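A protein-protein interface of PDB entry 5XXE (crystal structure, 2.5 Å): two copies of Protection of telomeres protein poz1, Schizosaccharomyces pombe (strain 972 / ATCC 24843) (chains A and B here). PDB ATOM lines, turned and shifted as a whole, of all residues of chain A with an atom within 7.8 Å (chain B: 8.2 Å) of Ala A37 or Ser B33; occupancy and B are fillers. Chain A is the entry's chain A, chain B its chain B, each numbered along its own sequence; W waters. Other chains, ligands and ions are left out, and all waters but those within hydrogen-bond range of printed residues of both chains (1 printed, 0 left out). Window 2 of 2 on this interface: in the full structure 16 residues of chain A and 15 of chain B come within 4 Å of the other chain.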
ATOM      1  N   VAL A  11     -14.899 -13.936 -21.294  1.00  0.00           N
ATOM      2  CA  VAL A  11     -14.878 -14.315 -19.877  1.00  0.00           C
ATOM      3  C   VAL A  11     -13.435 -14.386 -19.365  1.00  0.00           C
ATOM      4  O   VAL A  11     -13.130 -13.900 -18.275  1.00  0.00           O
ATOM      5  CB  VAL A  11     -15.609 -15.656 -19.652  1.00  0.00           C
ATOM      6  CG1 VAL A  11     -15.364 -16.212 -18.249  1.00  0.00           C
ATOM      7  CG2 VAL A  11     -17.111 -15.484 -19.893  1.00  0.00           C
ATOM      8  N   LEU A  15     -11.393 -12.180 -16.446  1.00  0.00           N
ATOM      9  CA  LEU A  15     -10.507 -12.744 -15.411  1.00  0.00           C
ATOM     10  C   LEU A  15      -9.149 -12.050 -15.398  1.00  0.00           C
ATOM     11  O   LEU A  15      -8.624 -11.758 -14.332  1.00  0.00           O
ATOM     12  CB  LEU A  15     -10.318 -14.261 -15.559  1.00  0.00           C
ATOM     13  CG  LEU A  15     -11.371 -15.152 -14.903  1.00  0.00           C
ATOM     14  CD1 LEU A  15     -11.058 -16.617 -15.172  1.00  0.00           C
ATOM     15  CD2 LEU A  15     -11.478 -14.893 -13.407  1.00  0.00           C
ATOM     16  N   GLU A  31     -15.598  -9.937  -4.976  1.00  0.00           N
ATOM     17  CA  GLU A  31     -15.253 -10.523  -6.271  1.00  0.00           C
ATOM     18  C   GLU A  31     -15.329 -12.048  -6.340  1.00  0.00           C
ATOM     19  O   GLU A  31     -15.126 -12.605  -7.414  1.00  0.00           O
ATOM     20  CB  GLU A  31     -13.840 -10.095  -6.656  1.00  0.00           C
ATOM     21  CG  GLU A  31     -13.513  -8.650  -6.310  1.00  0.00           C
ATOM     22  CD  GLU A  31     -12.230  -8.164  -6.951  1.00  0.00           C
ATOM     23  OE1 GLU A  31     -11.292  -8.981  -7.133  1.00  0.00           O
ATOM     24  OE2 GLU A  31     -12.170  -6.953  -7.267  1.00  0.00           O
ATOM     25  N   SER A  32     -15.614 -12.729  -5.230  1.00  0.00           N
ATOM     26  CA  SER A  32     -15.636 -14.202  -5.217  1.00  0.00           C
ATOM     27  C   SER A  32     -16.652 -14.759  -6.196  1.00  0.00           C
ATOM     28  O   SER A  32     -16.377 -15.727  -6.907  1.00  0.00           O
ATOM     29  CB  SER A  32     -15.969 -14.780  -3.828  1.00  0.00           C
ATOM     30  OG  SER A  32     -15.776 -13.834  -2.809  1.00  0.00           O
ATOM     31  N   SER A  33     -17.836 -14.156  -6.199  1.00  0.00           N
ATOM     32  CA  SER A  33     -18.958 -14.708  -6.925  1.00  0.00           C
ATOM     33  C   SER A  33     -18.725 -14.654  -8.433  1.00  0.00           C
ATOM     34  O   SER A  33     -18.969 -15.647  -9.124  1.00  0.00           O
ATOM     35  CB  SER A  33     -20.240 -13.990  -6.547  1.00  0.00           C
ATOM     36  OG  SER A  33     -21.342 -14.591  -7.202  1.00  0.00           O
ATOM     37  N   ILE A  34     -18.217 -13.522  -8.925  1.00  0.00           N
ATOM     38  CA  ILE A  34     -17.941 -13.376 -10.355  1.00  0.00           C
ATOM     39  C   ILE A  34     -16.723 -14.187 -10.811  1.00  0.00           C
ATOM     40  O   ILE A  34     -16.752 -14.802 -11.882  1.00  0.00           O
ATOM     41  CB  ILE A  34     -17.833 -11.887 -10.782  1.00  0.00           C
ATOM     42  CG1 ILE A  34     -17.936 -11.760 -12.304  1.00  0.00           C
ATOM     43  CG2 ILE A  34     -16.555 -11.225 -10.277  1.00  0.00           C
ATOM     44  CD1 ILE A  34     -18.123 -10.337 -12.764  1.00  0.00           C
ATOM     45  N   VAL A  35     -15.666 -14.189 -10.000  1.00  0.00           N
ATOM     46  CA  VAL A  35     -14.453 -14.968 -10.295  1.00  0.00           C
ATOM     47  C   VAL A  35     -14.783 -16.459 -10.341  1.00  0.00           C
ATOM     48  O   VAL A  35     -14.383 -17.147 -11.265  1.00  0.00           O
ATOM     49  CB  VAL A  35     -13.337 -14.704  -9.257  1.00  0.00           C
ATOM     50  CG1 VAL A  35     -12.188 -15.706  -9.394  1.00  0.00           C
ATOM     51  CG2 VAL A  35     -12.813 -13.273  -9.362  1.00  0.00           C
ATOM     52  N   ASN A  36     -15.514 -16.943  -9.345  1.00  0.00           N
ATOM     53  CA  ASN A  36     -16.008 -18.318  -9.360  1.00  0.00           C
ATOM     54  C   ASN A  36     -16.849 -18.610 -10.593  1.00  0.00           C
ATOM     55  O   ASN A  36     -16.669 -19.644 -11.223  1.00  0.00           O
ATOM     56  CB  ASN A  36     -16.831 -18.627  -8.098  1.00  0.00           C
ATOM     57  CG  ASN A  36     -15.970 -18.771  -6.852  1.00  0.00           C
ATOM     58  OD1 ASN A  36     -14.758 -18.950  -6.940  1.00  0.00           O
ATOM     59  ND2 ASN A  36     -16.596 -18.675  -5.684  1.00  0.00           N
ATOM     60  N   ALA A  37     -17.768 -17.704 -10.926  1.00  0.00           N
ATOM     61  CA  ALA A  37     -18.641 -17.874 -12.091  1.00  0.00           C
ATOM     62  C   ALA A  37     -17.849 -17.878 -13.401  1.00  0.00           C
ATOM     63  O   ALA A  37     -18.166 -18.647 -14.313  1.00  0.00           O
ATOM     64  CB  ALA A  37     -19.721 -16.806 -12.119  1.00  0.00           C
ATOM     65  N   CYS A  38     -16.822 -17.032 -13.483  1.00  0.00           N
ATOM     66  CA  CYS A  38     -15.905 -17.037 -14.632  1.00  0.00           C
ATOM     67  C   CYS A  38     -15.102 -18.352 -14.740  1.00  0.00           C
ATOM     68  O   CYS A  38     -14.973 -18.918 -15.834  1.00  0.00           O
ATOM     69  CB  CYS A  38     -14.936 -15.840 -14.579  1.00  0.00           C
ATOM     70  SG  CYS A  38     -15.672 -14.210 -14.866  1.00  0.00           S
ATOM     71  N   LEU A  39     -14.558 -18.819 -13.611  1.00  0.00           N
ATOM     72  CA  LEU A  39     -13.773 -20.053 -13.585  1.00  0.00           C
ATOM     73  C   LEU A  39     -14.637 -21.260 -13.914  1.00  0.00           C
ATOM     74  O   LEU A  39     -14.218 -22.124 -14.679  1.00  0.00           O
ATOM     75  CB  LEU A  39     -13.084 -20.265 -12.229  1.00  0.00           C
ATOM     76  CG  LEU A  39     -11.974 -19.286 -11.828  1.00  0.00           C
ATOM     77  CD1 LEU A  39     -11.626 -19.452 -10.355  1.00  0.00           C
ATOM     78  CD2 LEU A  39     -10.730 -19.455 -12.676  1.00  0.00           C
ATOM     79  N   ARG A  40     -15.836 -21.329 -13.342  1.00  0.00           N
ATOM     80  CA  ARG A  40     -16.760 -22.413 -13.678  1.00  0.00           C
ATOM     81  C   ARG A  40     -17.174 -22.401 -15.163  1.00  0.00           C
ATOM     82  O   ARG A  40     -17.336 -23.468 -15.766  1.00  0.00           O
ATOM     83  CB  ARG A  40     -18.005 -22.413 -12.781  1.00  0.00           C
ATOM     84  CG  ARG A  40     -18.690 -23.770 -12.815  1.00  0.00           C
ATOM     85  CD  ARG A  40     -20.045 -23.842 -12.137  1.00  0.00           C
ATOM     86  NE  ARG A  40     -20.544 -25.218 -12.214  1.00  0.00           N
ATOM     87  CZ  ARG A  40     -21.038 -25.806 -13.310  1.00  0.00           C
ATOM     88  NH1 ARG A  40     -21.148 -25.150 -14.471  1.00  0.00           N
ATOM     89  NH2 ARG A  40     -21.435 -27.077 -13.255  1.00  0.00           N
ATOM     90  N   TYR A  41     -17.323 -21.212 -15.752  1.00  0.00           N
ATOM     91  CA  TYR A  41     -17.731 -21.085 -17.154  1.00  0.00           C
ATOM     92  C   TYR A  41     -16.642 -21.585 -18.083  1.00  0.00           C
ATOM     93  O   TYR A  41     -16.928 -22.336 -19.015  1.00  0.00           O
ATOM     94  CB  TYR A  41     -18.103 -19.638 -17.510  1.00  0.00           C
ATOM     95  CG  TYR A  41     -18.791 -19.510 -18.852  1.00  0.00           C
ATOM     96  CD1 TYR A  41     -20.140 -19.813 -18.993  1.00  0.00           C
ATOM     97  CD2 TYR A  41     -18.088 -19.110 -19.981  1.00  0.00           C
ATOM     98  CE1 TYR A  41     -20.775 -19.721 -20.220  1.00  0.00           C
ATOM     99  CE2 TYR A  41     -18.712 -19.008 -21.213  1.00  0.00           C
ATOM    100  CZ  TYR A  41     -20.056 -19.316 -21.326  1.00  0.00           C
ATOM    101  OH  TYR A  41     -20.675 -19.212 -22.541  1.00  0.00           O
ATOM    102  N   LEU A  42     -15.402 -21.165 -17.833  1.00  0.00           N
ATOM    103  CA  LEU A  42     -14.241 -21.646 -18.604  1.00  0.00           C
ATOM    104  C   LEU A  42     -13.986 -23.126 -18.357  1.00  0.00           C
ATOM    105  O   LEU A  42     -13.636 -23.862 -19.278  1.00  0.00           O
ATOM    106  CB  LEU A  42     -12.985 -20.860 -18.241  1.00  0.00           C
ATOM    107  CG  LEU A  42     -12.978 -19.376 -18.605  1.00  0.00           C
ATOM    108  CD1 LEU A  42     -11.784 -18.698 -17.963  1.00  0.00           C
ATOM    109  CD2 LEU A  42     -12.952 -19.179 -20.109  1.00  0.00           C
ATOM    110  N   GLY A  43     -14.164 -23.550 -17.107  1.00  0.00           N
ATOM    111  CA  GLY A  43     -14.035 -24.951 -16.718  1.00  0.00           C
ATOM    112  C   GLY A  43     -14.964 -25.910 -17.440  1.00  0.00           C
ATOM    113  O   GLY A  43     -14.587 -27.048 -17.698  1.00  0.00           O
ATOM    114  N   PHE B  18     -22.805 -11.800 -24.220  1.00  0.00           N
ATOM    115  CA  PHE B  18     -23.886 -12.745 -23.853  1.00  0.00           C
ATOM    116  C   PHE B  18     -25.288 -12.260 -24.238  1.00  0.00           C
ATOM    117  O   PHE B  18     -26.188 -13.077 -24.437  1.00  0.00           O
ATOM    118  CB  PHE B  18     -23.898 -12.996 -22.330  1.00  0.00           C
ATOM    119  CG  PHE B  18     -22.933 -14.056 -21.865  1.00  0.00           C
ATOM    120  CD1 PHE B  18     -21.575 -13.819 -21.849  1.00  0.00           C
ATOM    121  CD2 PHE B  18     -23.397 -15.277 -21.411  1.00  0.00           C
ATOM    122  CE1 PHE B  18     -20.688 -14.787 -21.416  1.00  0.00           C
ATOM    123  CE2 PHE B  18     -22.522 -16.248 -20.969  1.00  0.00           C
ATOM    124  CZ  PHE B  18     -21.160 -16.001 -20.972  1.00  0.00           C
ATOM    125  N   MET B  27     -32.507 -16.197 -20.984  1.00  0.00           N
ATOM    126  CA  MET B  27     -31.602 -16.811 -20.008  1.00  0.00           C
ATOM    127  C   MET B  27     -31.507 -18.291 -20.233  1.00  0.00           C
ATOM    128  O   MET B  27     -32.482 -18.995 -20.038  1.00  0.00           O
ATOM    129  CB  MET B  27     -32.135 -16.654 -18.582  1.00  0.00           C
ATOM    130  CG  MET B  27     -31.900 -15.281 -17.967  1.00  0.00           C
ATOM    131  SD  MET B  27     -30.531 -15.355 -16.556  1.00  0.00           S
ATOM    132  CE  MET B  27     -29.145 -16.072 -17.758  1.00  0.00           C
ATOM    133  N   GLN B  28     -30.338 -18.779 -20.633  1.00  0.00           N
ATOM    134  CA  GLN B  28     -30.073 -20.223 -20.708  1.00  0.00           C
ATOM    135  C   GLN B  28     -29.468 -20.701 -19.377  1.00  0.00           C
ATOM    136  O   GLN B  28     -28.672 -19.984 -18.770  1.00  0.00           O
ATOM    137  CB  GLN B  28     -29.100 -20.531 -21.851  1.00  0.00           C
ATOM    138  CG  GLN B  28     -29.463 -19.945 -23.214  1.00  0.00           C
ATOM    139  CD  GLN B  28     -30.765 -20.495 -23.756  1.00  0.00           C
ATOM    140  OE1 GLN B  28     -30.878 -21.694 -24.009  1.00  0.00           O
ATOM    141  NE2 GLN B  28     -31.758 -19.620 -23.941  1.00  0.00           N
ATOM    142  N   ARG B  29     -29.836 -21.904 -18.936  1.00  0.00           N
ATOM    143  CA  ARG B  29     -29.290 -22.518 -17.698  1.00  0.00           C
ATOM    144  C   ARG B  29     -27.777 -22.374 -17.492  1.00  0.00           C
ATOM    145  O   ARG B  29     -27.336 -21.962 -16.429  1.00  0.00           O
ATOM    146  CB  ARG B  29     -29.640 -24.017 -17.613  1.00  0.00           C
ATOM    147  CG  ARG B  29     -30.873 -24.344 -16.772  1.00  0.00           C
ATOM    148  CD  ARG B  29     -30.558 -25.355 -15.669  1.00  0.00           C
ATOM    149  NE  ARG B  29     -31.626 -25.419 -14.661  1.00  0.00           N
ATOM    150  CZ  ARG B  29     -31.471 -25.750 -13.373  1.00  0.00           C
ATOM    151  NH1 ARG B  29     -30.274 -26.058 -12.862  1.00  0.00           N
ATOM    152  NH2 ARG B  29     -32.535 -25.762 -12.571  1.00  0.00           N
ATOM    153  N   GLU B  30     -26.997 -22.701 -18.517  1.00  0.00           N
ATOM    154  CA  GLU B  30     -25.526 -22.712 -18.422  1.00  0.00           C
ATOM    155  C   GLU B  30     -24.879 -21.321 -18.363  1.00  0.00           C
ATOM    156  O   GLU B  30     -23.679 -21.207 -18.103  1.00  0.00           O
ATOM    157  CB  GLU B  30     -24.933 -23.526 -19.580  1.00  0.00           C
ATOM    158  CG  GLU B  30     -25.337 -25.002 -19.528  1.00  0.00           C
ATOM    159  CD  GLU B  30     -25.000 -25.800 -20.789  1.00  0.00           C
ATOM    160  OE1 GLU B  30     -24.264 -25.295 -21.671  1.00  0.00           O
ATOM    161  OE2 GLU B  30     -25.479 -26.957 -20.889  1.00  0.00           O
ATOM    162  N   GLU B  31     -25.672 -20.276 -18.617  1.00  0.00           N
ATOM    163  CA  GLU B  31     -25.242 -18.877 -18.485  1.00  0.00           C
ATOM    164  C   GLU B  31     -25.843 -18.145 -17.270  1.00  0.00           C
ATOM    165  O   GLU B  31     -25.364 -17.080 -16.933  1.00  0.00           O
ATOM    166  CB  GLU B  31     -25.583 -18.126 -19.774  1.00  0.00           C
ATOM    167  CG  GLU B  31     -25.153 -18.862 -21.046  1.00  0.00           C
ATOM    168  CD  GLU B  31     -25.500 -18.131 -22.335  1.00  0.00           C
ATOM    169  OE1 GLU B  31     -26.103 -17.030 -22.274  1.00  0.00           O
ATOM    170  OE2 GLU B  31     -25.165 -18.669 -23.422  1.00  0.00           O
ATOM    171  N   SER B  32     -26.872 -18.708 -16.626  1.00  0.00           N
ATOM    172  CA  SER B  32     -27.528 -18.115 -15.437  1.00  0.00           C
ATOM    173  C   SER B  32     -26.575 -17.498 -14.424  1.00  0.00           C
ATOM    174  O   SER B  32     -26.767 -16.366 -13.975  1.00  0.00           O
ATOM    175  CB  SER B  32     -28.348 -19.164 -14.674  1.00  0.00           C
ATOM    176  OG  SER B  32     -29.476 -19.578 -15.403  1.00  0.00           O
ATOM    177  N   SER B  33     -25.566 -18.282 -14.065  1.00  0.00           N
ATOM    178  CA  SER B  33     -24.698 -17.985 -12.954  1.00  0.00           C
ATOM    179  C   SER B  33     -23.758 -16.831 -13.310  1.00  0.00           C
ATOM    180  O   SER B  33     -23.614 -15.884 -12.532  1.00  0.00           O
ATOM    181  CB  SER B  33     -23.938 -19.258 -12.552  1.00  0.00           C
ATOM    182  OG  SER B  33     -22.939 -18.991 -11.589  1.00  0.00           O
ATOM    183  N   ILE B  34     -23.151 -16.886 -14.488  1.00  0.00           N
ATOM    184  CA  ILE B  34     -22.239 -15.828 -14.892  1.00  0.00           C
ATOM    185  C   ILE B  34     -22.977 -14.537 -15.246  1.00  0.00           C
ATOM    186  O   ILE B  34     -22.484 -13.452 -14.933  1.00  0.00           O
ATOM    187  CB  ILE B  34     -21.255 -16.268 -16.007  1.00  0.00           C
ATOM    188  CG1 ILE B  34     -20.092 -15.279 -16.086  1.00  0.00           C
ATOM    189  CG2 ILE B  34     -21.943 -16.406 -17.357  1.00  0.00           C
ATOM    190  CD1 ILE B  34     -18.999 -15.731 -17.016  1.00  0.00           C
ATOM    191  N   VAL B  35     -24.149 -14.647 -15.869  1.00  0.00           N
ATOM    192  CA  VAL B  35     -24.982 -13.467 -16.140  1.00  0.00           C
ATOM    193  C   VAL B  35     -25.446 -12.809 -14.835  1.00  0.00           C
ATOM    194  O   VAL B  35     -25.360 -11.587 -14.702  1.00  0.00           O
ATOM    195  CB  VAL B  35     -26.180 -13.803 -17.057  1.00  0.00           C
ATOM    196  CG1 VAL B  35     -27.213 -12.679 -17.079  1.00  0.00           C
ATOM    197  CG2 VAL B  35     -25.694 -14.089 -18.467  1.00  0.00           C
ATOM    198  N   ASN B  36     -25.924 -13.610 -13.886  1.00  0.00           N
ATOM    199  CA  ASN B  36     -26.314 -13.092 -12.571  1.00  0.00           C
ATOM    200  C   ASN B  36     -25.171 -12.458 -11.801  1.00  0.00           C
ATOM    201  O   ASN B  36     -25.369 -11.449 -11.119  1.00  0.00           O
ATOM    202  CB  ASN B  36     -26.943 -14.186 -11.711  1.00  0.00           C
ATOM    203  CG  ASN B  36     -28.362 -14.510 -12.128  1.00  0.00           C
ATOM    204  OD1 ASN B  36     -28.992 -13.761 -12.866  1.00  0.00           O
ATOM    205  ND2 ASN B  36     -28.878 -15.622 -11.640  1.00  0.00           N
ATOM    206  N   ALA B  37     -23.981 -13.045 -11.913  1.00  0.00           N
ATOM    207  CA  ALA B  37     -22.802 -12.525 -11.232  1.00  0.00           C
ATOM    208  C   ALA B  37     -22.320 -11.219 -11.853  1.00  0.00           C
ATOM    209  O   ALA B  37     -21.960 -10.286 -11.127  1.00  0.00           O
ATOM    210  CB  ALA B  37     -21.684 -13.561 -11.219  1.00  0.00           C
ATOM    211  N   CYS B  38     -22.302 -11.151 -13.184  1.00  0.00           N
ATOM    212  CA  CYS B  38     -21.977  -9.900 -13.872  1.00  0.00           C
ATOM    213  C   CYS B  38     -22.975  -8.779 -13.526  1.00  0.00           C
ATOM    214  O   CYS B  38     -22.559  -7.678 -13.223  1.00  0.00           O
ATOM    215  CB  CYS B  38     -21.919 -10.107 -15.383  1.00  0.00           C
ATOM    216  SG  CYS B  38     -20.570 -11.174 -15.950  1.00  0.00           S
ATOM    217  N   LEU B  39     -24.278  -9.068 -13.552  1.00  0.00           N
ATOM    218  CA  LEU B  39     -25.309  -8.066 -13.212  1.00  0.00           C
ATOM    219  C   LEU B  39     -25.212  -7.558 -11.770  1.00  0.00           C
ATOM    220  O   LEU B  39     -25.397  -6.367 -11.520  1.00  0.00           O
ATOM    221  CB  LEU B  39     -26.723  -8.607 -13.455  1.00  0.00           C
ATOM    222  CG  LEU B  39     -27.185  -8.730 -14.904  1.00  0.00           C
ATOM    223  CD1 LEU B  39     -28.467  -9.532 -14.970  1.00  0.00           C
ATOM    224  CD2 LEU B  39     -27.406  -7.366 -15.522  1.00  0.00           C
ATOM    225  N   ARG B  40     -24.936  -8.463 -10.829  1.00  0.00           N
ATOM    226  CA  ARG B  40     -24.715  -8.071  -9.428  1.00  0.00           C
ATOM    227  C   ARG B  40     -23.431  -7.268  -9.263  1.00  0.00           C
ATOM    228  O   ARG B  40     -23.424  -6.276  -8.555  1.00  0.00           O
ATOM    229  CB  ARG B  40     -24.717  -9.267  -8.472  1.00  0.00           C
ATOM    230  CG  ARG B  40     -25.070  -8.872  -7.042  1.00  0.00           C
ATOM    231  CD  ARG B  40     -24.766  -9.979  -6.044  1.00  0.00           C
ATOM    232  NE  ARG B  40     -25.209  -9.640  -4.686  1.00  0.00           N
ATOM    233  CZ  ARG B  40     -24.591  -8.796  -3.856  1.00  0.00           C
ATOM    234  NH1 ARG B  40     -23.476  -8.159  -4.207  1.00  0.00           N
ATOM    235  NH2 ARG B  40     -25.103  -8.574  -2.652  1.00  0.00           N
HETATM  236  O   HOH W   1     -22.686 -20.764 -23.136  1.00  0.00           O
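The backbone carbonyl oxygen (O) of Ile A34 is in hydrogen-bond range of the side-chain sulfur (SG) of Cys A38.
The side-chain sulfur (SG) of Cys B38 sits at hydrogen-bond distance from the backbone carbonyl oxygen (O) of Ile B34 (3.1 Å).
Printed residues of chain A that touch a printed residue of chain B: Val A11, Ile A34, Ala A37 and Tyr A41.
Hydrophobic or aromatic side chains of chain A within 4 Å of the printed part of chain B: Val A11, Ala A37 and Tyr A41.
Among the printed residues, no Asp or Glu carboxylate lies within 4 Å of a Lys or Arg side-chain nitrogen of the other chain.
Of chain B, only Ser B33 (3.9 Å), Ile B34 (3.9 Å) and Ala B37 (3.9 Å) come within 4 Å of Ala A37.
Of chain A, only Ala A37 (3.9 Å) comes within 4 Å of Ser B33.
Of the printed residues of chain A, Glu B30 touches Tyr A41 (3.9 Å).
Of the printed residues of chain A, Ala B37 touches Ile A34 (3.8 Å) and Ala A37 (3.9 Å).
Printed residues of chain A within 4 Å of Ile B34: Val A11 and Ala A37.
Printed residues of chain A within 4 Å of Phe B18: Val A11 (3.9 Å) and Tyr A41 (3.5 Å).
Of the printed residues of chain B, Tyr A41 touches Phe B18 (3.5 Å) and Glu B30 (3.9 Å).
Leu A39 touches none of the printed residues of chain B.
Leu A42 touches none of the printed residues of chain B.
The nearest residue of chain B that does not touch Ala A37 is Val B35 (6.2 Å).
Ile A34 touches Ala B37, and with the chains exchanged Ala A37 touches Ile B34.
Ala A37 touches Ser B33, but with the chains exchanged Ser A33 does not touch Ala B37 (4.01 Å).
Ala A37 touches its own counterpart, Ala B37.
10 positions are printed for both chains.
Of the 8 pairs that touch across the chains among the printed residues, 3 have their exchanged pair printed and touching as well.
Water W1 bridges OH of Tyr A41 (2.6 Å) and OE2 of Glu B31 (3.3 Å).
Among the printed residues, merely in contact across the chains: Val A11 with Phe B18 (3.9 Å), Val A11 with Ile B34 (3.5 Å), Ile A34 with Ala B37 (3.8 Å), Ala A37 with Ser B33 (3.9 Å), Ala A37 with Ile B34 (3.9 Å), Ala A37 with Ala B37 (3.9 Å), Tyr A41 with Phe B18 (3.5 Å) and Tyr A41 with Glu B30 (3.9 Å).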
